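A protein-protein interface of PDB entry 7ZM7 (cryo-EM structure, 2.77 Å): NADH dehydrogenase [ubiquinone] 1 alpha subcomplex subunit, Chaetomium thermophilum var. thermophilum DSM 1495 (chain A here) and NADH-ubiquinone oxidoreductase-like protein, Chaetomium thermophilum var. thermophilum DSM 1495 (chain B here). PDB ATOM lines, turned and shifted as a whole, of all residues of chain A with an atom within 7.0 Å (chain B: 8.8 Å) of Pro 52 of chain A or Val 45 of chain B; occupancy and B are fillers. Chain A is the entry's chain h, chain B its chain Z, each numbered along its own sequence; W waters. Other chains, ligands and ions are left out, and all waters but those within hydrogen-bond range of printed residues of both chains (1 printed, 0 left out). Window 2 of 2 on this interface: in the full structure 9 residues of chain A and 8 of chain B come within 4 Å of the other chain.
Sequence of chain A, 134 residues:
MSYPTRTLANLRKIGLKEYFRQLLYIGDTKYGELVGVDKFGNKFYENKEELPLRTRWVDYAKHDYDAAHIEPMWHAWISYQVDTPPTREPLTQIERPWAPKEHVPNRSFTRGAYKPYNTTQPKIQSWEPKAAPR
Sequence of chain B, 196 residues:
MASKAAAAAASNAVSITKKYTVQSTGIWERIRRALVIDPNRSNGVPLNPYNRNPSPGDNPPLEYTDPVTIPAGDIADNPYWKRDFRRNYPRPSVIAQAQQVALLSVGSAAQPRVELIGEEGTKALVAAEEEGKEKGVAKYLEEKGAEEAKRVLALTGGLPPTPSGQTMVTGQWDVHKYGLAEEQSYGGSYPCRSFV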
ATOM      1  N   GLU A  50      12.775  -7.305 -24.225  1.00  0.00           N
ATOM      2  CA  GLU A  50      14.210  -7.496 -24.269  1.00  0.00           C
ATOM      3  C   GLU A  50      14.531  -8.989 -24.265  1.00  0.00           C
ATOM      4  O   GLU A  50      13.652  -9.843 -24.397  1.00  0.00           O
ATOM      5  CB  GLU A  50      14.857  -6.727 -23.127  1.00  0.00           C
ATOM      6  CG  GLU A  50      14.779  -5.255 -23.372  1.00  0.00           C
ATOM      7  CD  GLU A  50      15.770  -4.457 -22.578  1.00  0.00           C
ATOM      8  OE1 GLU A  50      15.339  -3.704 -21.696  1.00  0.00           O
ATOM      9  OE2 GLU A  50      16.986  -4.578 -22.833  1.00  0.00           O
ATOM     10  N   LEU A  51      15.798  -9.319 -24.162  1.00  0.00           N
ATOM     11  CA  LEU A  51      16.166 -10.711 -24.064  1.00  0.00           C
ATOM     12  C   LEU A  51      15.770 -11.252 -22.701  1.00  0.00           C
ATOM     13  O   LEU A  51      15.678 -10.504 -21.733  1.00  0.00           O
ATOM     14  CB  LEU A  51      17.657 -10.865 -24.312  1.00  0.00           C
ATOM     15  CG  LEU A  51      18.026 -10.518 -25.748  1.00  0.00           C
ATOM     16  CD1 LEU A  51      19.429 -10.964 -26.074  1.00  0.00           C
ATOM     17  CD2 LEU A  51      17.053 -11.172 -26.708  1.00  0.00           C
ATOM     18  N   PRO A  52      15.497 -12.549 -22.604  1.00  0.00           N
ATOM     19  CA  PRO A  52      15.027 -13.095 -21.335  1.00  0.00           C
ATOM     20  C   PRO A  52      16.060 -12.896 -20.246  1.00  0.00           C
ATOM     21  O   PRO A  52      17.260 -13.045 -20.476  1.00  0.00           O
ATOM     22  CB  PRO A  52      14.815 -14.574 -21.653  1.00  0.00           C
ATOM     23  CG  PRO A  52      14.625 -14.608 -23.110  1.00  0.00           C
ATOM     24  CD  PRO A  52      15.540 -13.585 -23.646  1.00  0.00           C
ATOM     25  N   LEU A  53      15.574 -12.561 -19.055  1.00  0.00           N
ATOM     26  CA  LEU A  53      16.317 -12.211 -17.852  1.00  0.00           C
ATOM     27  C   LEU A  53      16.842 -10.783 -17.922  1.00  0.00           C
ATOM     28  O   LEU A  53      17.500 -10.332 -16.994  1.00  0.00           O
ATOM     29  CB  LEU A  53      17.489 -13.162 -17.568  1.00  0.00           C
ATOM     30  CG  LEU A  53      17.238 -14.663 -17.638  1.00  0.00           C
ATOM     31  CD1 LEU A  53      18.405 -15.354 -17.094  1.00  0.00           C
ATOM     32  CD2 LEU A  53      15.999 -15.057 -16.892  1.00  0.00           C
ATOM     33  N   ARG A  54      16.568 -10.059 -18.996  1.00  0.00           N
ATOM     34  CA  ARG A  54      16.947  -8.670 -19.112  1.00  0.00           C
ATOM     35  C   ARG A  54      15.749  -7.746 -19.123  1.00  0.00           C
ATOM     36  O   ARG A  54      15.921  -6.553 -19.386  1.00  0.00           O
ATOM     37  CB  ARG A  54      17.774  -8.444 -20.381  1.00  0.00           C
ATOM     38  CG  ARG A  54      18.761  -9.537 -20.675  1.00  0.00           C
ATOM     39  CD  ARG A  54      19.813  -9.049 -21.613  1.00  0.00           C
ATOM     40  NE  ARG A  54      20.280  -7.729 -21.236  1.00  0.00           N
ATOM     41  CZ  ARG A  54      21.151  -7.010 -21.934  1.00  0.00           C
ATOM     42  NH1 ARG A  54      21.505  -5.811 -21.506  1.00  0.00           N
ATOM     43  NH2 ARG A  54      21.659  -7.485 -23.054  1.00  0.00           N
ATOM     44  N   THR A  55      14.548  -8.259 -18.844  1.00  0.00           N
ATOM     45  CA  THR A  55      13.348  -7.432 -18.863  1.00  0.00           C
ATOM     46  C   THR A  55      13.279  -6.477 -17.679  1.00  0.00           C
ATOM     47  O   THR A  55      12.547  -5.492 -17.735  1.00  0.00           O
ATOM     48  CB  THR A  55      12.090  -8.301 -18.882  1.00  0.00           C
ATOM     49  OG1 THR A  55      12.033  -9.088 -17.689  1.00  0.00           O
ATOM     50  CG2 THR A  55      12.081  -9.216 -20.080  1.00  0.00           C
ATOM     51  N   TYR A  80      13.136 -11.885 -10.424  1.00  0.00           N
ATOM     52  CA  TYR A  80      12.077 -12.637 -11.075  1.00  0.00           C
ATOM     53  C   TYR A  80      11.428 -13.622 -10.133  1.00  0.00           C
ATOM     54  O   TYR A  80      10.873 -14.625 -10.570  1.00  0.00           O
ATOM     55  CB  TYR A  80      12.582 -13.341 -12.337  1.00  0.00           C
ATOM     56  CG  TYR A  80      12.998 -12.368 -13.397  1.00  0.00           C
ATOM     57  CD1 TYR A  80      14.296 -11.878 -13.438  1.00  0.00           C
ATOM     58  CD2 TYR A  80      12.095 -11.914 -14.342  1.00  0.00           C
ATOM     59  CE1 TYR A  80      14.683 -10.974 -14.386  1.00  0.00           C
ATOM     60  CE2 TYR A  80      12.483 -11.007 -15.301  1.00  0.00           C
ATOM     61  CZ  TYR A  80      13.784 -10.548 -15.316  1.00  0.00           C
ATOM     62  OH  TYR A  80      14.192  -9.657 -16.258  1.00  0.00           O
ATOM     63  N   LYS B  19       9.026 -24.603 -32.158  1.00  0.00           N
ATOM     64  CA  LYS B  19      10.163 -24.881 -31.294  1.00  0.00           C
ATOM     65  C   LYS B  19      10.322 -23.948 -30.104  1.00  0.00           C
ATOM     66  O   LYS B  19      11.310 -24.082 -29.382  1.00  0.00           O
ATOM     67  CB  LYS B  19      11.459 -24.897 -32.098  1.00  0.00           C
ATOM     68  CG  LYS B  19      11.822 -26.266 -32.591  1.00  0.00           C
ATOM     69  CD  LYS B  19      13.140 -26.268 -33.287  1.00  0.00           C
ATOM     70  CE  LYS B  19      13.296 -27.544 -34.052  1.00  0.00           C
ATOM     71  NZ  LYS B  19      14.684 -27.738 -34.465  1.00  0.00           N
ATOM     72  N   TYR B  20       9.384 -23.044 -29.849  1.00  0.00           N
ATOM     73  CA  TYR B  20       9.368 -22.256 -28.606  1.00  0.00           C
ATOM     74  C   TYR B  20      10.687 -21.534 -28.379  1.00  0.00           C
ATOM     75  O   TYR B  20      11.305 -21.631 -27.325  1.00  0.00           O
ATOM     76  CB  TYR B  20       9.027 -23.113 -27.391  1.00  0.00           C
ATOM     77  CG  TYR B  20       7.614 -23.594 -27.378  1.00  0.00           C
ATOM     78  CD1 TYR B  20       6.591 -22.800 -26.901  1.00  0.00           C
ATOM     79  CD2 TYR B  20       7.302 -24.843 -27.844  1.00  0.00           C
ATOM     80  CE1 TYR B  20       5.316 -23.242 -26.897  1.00  0.00           C
ATOM     81  CE2 TYR B  20       6.034 -25.292 -27.835  1.00  0.00           C
ATOM     82  CZ  TYR B  20       5.038 -24.496 -27.372  1.00  0.00           C
ATOM     83  OH  TYR B  20       3.761 -24.990 -27.384  1.00  0.00           O
ATOM     84  N   THR B  21      11.144 -20.854 -29.410  1.00  0.00           N
ATOM     85  CA  THR B  21      12.271 -19.951 -29.345  1.00  0.00           C
ATOM     86  C   THR B  21      11.902 -18.708 -30.130  1.00  0.00           C
ATOM     87  O   THR B  21      10.983 -18.723 -30.952  1.00  0.00           O
ATOM     88  CB  THR B  21      13.568 -20.575 -29.902  1.00  0.00           C
ATOM     89  OG1 THR B  21      13.530 -20.575 -31.330  1.00  0.00           O
ATOM     90  CG2 THR B  21      13.759 -21.976 -29.422  1.00  0.00           C
ATOM     91  N   VAL B  22      12.612 -17.618 -29.843  1.00  0.00           N
ATOM     92  CA  VAL B  22      12.386 -16.377 -30.565  1.00  0.00           C
ATOM     93  C   VAL B  22      12.693 -16.581 -32.036  1.00  0.00           C
ATOM     94  O   VAL B  22      13.654 -17.259 -32.412  1.00  0.00           O
ATOM     95  CB  VAL B  22      13.228 -15.247 -29.960  1.00  0.00           C
ATOM     96  CG1 VAL B  22      12.835 -13.932 -30.560  1.00  0.00           C
ATOM     97  CG2 VAL B  22      13.028 -15.217 -28.477  1.00  0.00           C
ATOM     98  N   GLN B  23      11.853 -16.013 -32.877  1.00  0.00           N
ATOM     99  CA  GLN B  23      11.936 -16.209 -34.307  1.00  0.00           C
ATOM    100  C   GLN B  23      12.468 -14.953 -34.973  1.00  0.00           C
ATOM    101  O   GLN B  23      12.370 -13.850 -34.440  1.00  0.00           O
ATOM    102  CB  GLN B  23      10.566 -16.572 -34.855  1.00  0.00           C
ATOM    103  CG  GLN B  23       9.881 -17.694 -34.107  1.00  0.00           C
ATOM    104  CD  GLN B  23      10.257 -19.066 -34.624  1.00  0.00           C
ATOM    105  OE1 GLN B  23       9.863 -19.451 -35.719  1.00  0.00           O
ATOM    106  NE2 GLN B  23      11.002 -19.815 -33.833  1.00  0.00           N
ATOM    107  N   SER B  42      16.759 -23.841 -34.023  1.00  0.00           N
ATOM    108  CA  SER B  42      16.487 -22.725 -33.140  1.00  0.00           C
ATOM    109  C   SER B  42      17.787 -22.064 -32.688  1.00  0.00           C
ATOM    110  O   SER B  42      18.884 -22.567 -32.924  1.00  0.00           O
ATOM    111  CB  SER B  42      15.678 -23.224 -31.957  1.00  0.00           C
ATOM    112  OG  SER B  42      16.367 -24.248 -31.274  1.00  0.00           O
ATOM    113  N   ASN B  43      17.663 -20.908 -32.051  1.00  0.00           N
ATOM    114  CA  ASN B  43      18.831 -20.223 -31.523  1.00  0.00           C
ATOM    115  C   ASN B  43      18.949 -20.343 -30.015  1.00  0.00           C
ATOM    116  O   ASN B  43      19.897 -19.811 -29.440  1.00  0.00           O
ATOM    117  CB  ASN B  43      18.830 -18.749 -31.924  1.00  0.00           C
ATOM    118  CG  ASN B  43      17.571 -18.052 -31.551  1.00  0.00           C
ATOM    119  OD1 ASN B  43      16.643 -18.657 -31.035  1.00  0.00           O
ATOM    120  ND2 ASN B  43      17.520 -16.765 -31.824  1.00  0.00           N
ATOM    121  N   GLY B  44      18.026 -21.044 -29.370  1.00  0.00           N
ATOM    122  CA  GLY B  44      18.086 -21.279 -27.953  1.00  0.00           C
ATOM    123  C   GLY B  44      17.599 -20.143 -27.087  1.00  0.00           C
ATOM    124  O   GLY B  44      17.698 -20.236 -25.861  1.00  0.00           O
ATOM    125  N   VAL B  45      17.093 -19.069 -27.673  1.00  0.00           N
ATOM    126  CA  VAL B  45      16.617 -17.917 -26.920  1.00  0.00           C
ATOM    127  C   VAL B  45      15.157 -18.172 -26.559  1.00  0.00           C
ATOM    128  O   VAL B  45      14.336 -18.346 -27.466  1.00  0.00           O
ATOM    129  CB  VAL B  45      16.776 -16.621 -27.721  1.00  0.00           C
ATOM    130  CG1 VAL B  45      16.237 -15.459 -26.943  1.00  0.00           C
ATOM    131  CG2 VAL B  45      18.219 -16.402 -28.056  1.00  0.00           C
ATOM    132  N   PRO B  46      14.805 -18.220 -25.281  1.00  0.00           N
ATOM    133  CA  PRO B  46      13.426 -18.540 -24.897  1.00  0.00           C
ATOM    134  C   PRO B  46      12.489 -17.364 -25.108  1.00  0.00           C
ATOM    135  O   PRO B  46      12.887 -16.234 -25.370  1.00  0.00           O
ATOM    136  CB  PRO B  46      13.549 -18.893 -23.415  1.00  0.00           C
ATOM    137  CG  PRO B  46      15.002 -19.052 -23.167  1.00  0.00           C
ATOM    138  CD  PRO B  46      15.698 -18.177 -24.120  1.00  0.00           C
ATOM    139  N   LEU B  47      11.205 -17.652 -24.977  1.00  0.00           N
ATOM    140  CA  LEU B  47      10.146 -16.688 -25.237  1.00  0.00           C
ATOM    141  C   LEU B  47       9.693 -16.037 -23.949  1.00  0.00           C
ATOM    142  O   LEU B  47       9.360 -16.730 -22.987  1.00  0.00           O
ATOM    143  CB  LEU B  47       8.964 -17.371 -25.901  1.00  0.00           C
ATOM    144  CG  LEU B  47       9.353 -18.058 -27.181  1.00  0.00           C
ATOM    145  CD1 LEU B  47       8.277 -19.021 -27.524  1.00  0.00           C
ATOM    146  CD2 LEU B  47       9.525 -17.025 -28.251  1.00  0.00           C
ATOM    147  N   ASN B  48       9.671 -14.709 -23.943  1.00  0.00           N
ATOM    148  CA  ASN B  48       9.286 -13.971 -22.743  1.00  0.00           C
ATOM    149  C   ASN B  48       7.844 -14.195 -22.324  1.00  0.00           C
ATOM    150  O   ASN B  48       7.602 -14.378 -21.123  1.00  0.00           O
ATOM    151  CB  ASN B  48       9.579 -12.483 -22.941  1.00  0.00           C
ATOM    152  CG  ASN B  48      10.954 -12.111 -22.522  1.00  0.00           C
ATOM    153  OD1 ASN B  48      11.603 -12.834 -21.782  1.00  0.00           O
ATOM    154  ND2 ASN B  48      11.416 -10.981 -22.993  1.00  0.00           N
ATOM    155  N   PRO B  49       6.848 -14.162 -23.212  1.00  0.00           N
ATOM    156  CA  PRO B  49       5.468 -14.346 -22.751  1.00  0.00           C
ATOM    157  C   PRO B  49       5.122 -15.762 -22.336  1.00  0.00           C
ATOM    158  O   PRO B  49       4.009 -15.981 -21.857  1.00  0.00           O
ATOM    159  CB  PRO B  49       4.646 -13.915 -23.965  1.00  0.00           C
ATOM    160  CG  PRO B  49       5.532 -14.133 -25.098  1.00  0.00           C
ATOM    161  CD  PRO B  49       6.881 -13.786 -24.637  1.00  0.00           C
ATOM    162  N   ASN B  51       7.822 -18.440 -21.172  1.00  0.00           N
ATOM    163  CA  ASN B  51       8.792 -19.194 -20.401  1.00  0.00           C
ATOM    164  C   ASN B  51       8.889 -18.627 -19.003  1.00  0.00           C
ATOM    165  O   ASN B  51       9.171 -17.440 -18.833  1.00  0.00           O
ATOM    166  CB  ASN B  51      10.161 -19.157 -21.070  1.00  0.00           C
ATOM    167  CG  ASN B  51      11.039 -20.276 -20.625  1.00  0.00           C
ATOM    168  OD1 ASN B  51      11.888 -20.112 -19.752  1.00  0.00           O
ATOM    169  ND2 ASN B  51      10.843 -21.437 -21.220  1.00  0.00           N
ATOM    170  N   ARG B  52       8.668 -19.487 -18.011  1.00  0.00           N
ATOM    171  CA  ARG B  52       8.689 -19.109 -16.607  1.00  0.00           C
ATOM    172  C   ARG B  52       7.760 -17.932 -16.356  1.00  0.00           C
ATOM    173  O   ARG B  52       8.039 -17.067 -15.534  1.00  0.00           O
ATOM    174  CB  ARG B  52      10.115 -18.809 -16.135  1.00  0.00           C
ATOM    175  CG  ARG B  52      10.334 -18.907 -14.649  1.00  0.00           C
ATOM    176  CD  ARG B  52      11.764 -18.593 -14.305  1.00  0.00           C
ATOM    177  NE  ARG B  52      12.031 -18.678 -12.877  1.00  0.00           N
ATOM    178  CZ  ARG B  52      11.799 -17.695 -12.017  1.00  0.00           C
ATOM    179  NH1 ARG B  52      11.265 -16.569 -12.425  1.00  0.00           N
ATOM    180  NH2 ARG B  52      12.081 -17.848 -10.746  1.00  0.00           N
HETATM  181  O   HOH W   1      12.490 -12.407 -18.819  1.00  0.00           O
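The backbone carbonyl oxygen of Glu 50 of chain A sits at hydrogen-bond distance from the side-chain amide nitrogen of Asn 48 of chain B (2.9 Å).
NH1 of Arg 52 of chain B lies within hydrogen-bond range of O of Tyr 80 of chain A (2.7 Å).
The backbone NH of Val 22 of chain B lies within hydrogen-bond range of the backbone carbonyl oxygen of Val 45 of chain B (3.0 Å).
N of Val 45 of chain B lies close to OD1 of Asn 43 of chain B, 3.4 Å away.
O of Leu 53 of chain A lies close to OH of Tyr 80 of chain A, 3.5 Å away.
OG1 of Thr 55 of chain A sits at hydrogen-bond distance from OH of Tyr 80 of chain A.
Val 45 of chain B touches Pro 52 of chain A (CG1 to CD, 3.9 Å).
Pro 46 of chain B touches Pro 52 of chain A (O to CG, 3.3 Å).
Pro 52 of chain A touches Asn 48 of chain B (CA to OD1, 3.5 Å).
ND2 of Asn 48 of chain B touches CG2 of Thr 55 of chain A, at 3.5 Å.
Of the printed residues of chain B, Pro 52 of chain A touches Val 45, Pro 46 and Asn 48.
Val 45 of chain B touches just one residue of chain A: Pro 52 (3.9 Å).
No residue of chain A comes within 4 Å of Gly 44 of chain B.
Of the printed residues of chain A, Arg 52 of chain B touches Tyr 80 (2.7 Å).
Printed residues of chain B within 4 Å of Tyr 80 of chain A: Arg 52.
Thr 21 of chain B touches none of the printed residues of chain A.
The nearest residue of chain B that does not touch Pro 52 of chain A is Leu 47 of chain B (4.9 Å).
Hydrophobic or aromatic side chains of chain B that line the printed part of chain A: Val 45 and Pro 46.
Water W1 lies within hydrogen-bond range of the backbone NH (N) of Leu 53 of chain A (3.1 Å) and the side-chain amide oxygen (OD1) of Asn 48 of chain B (3.1 Å).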
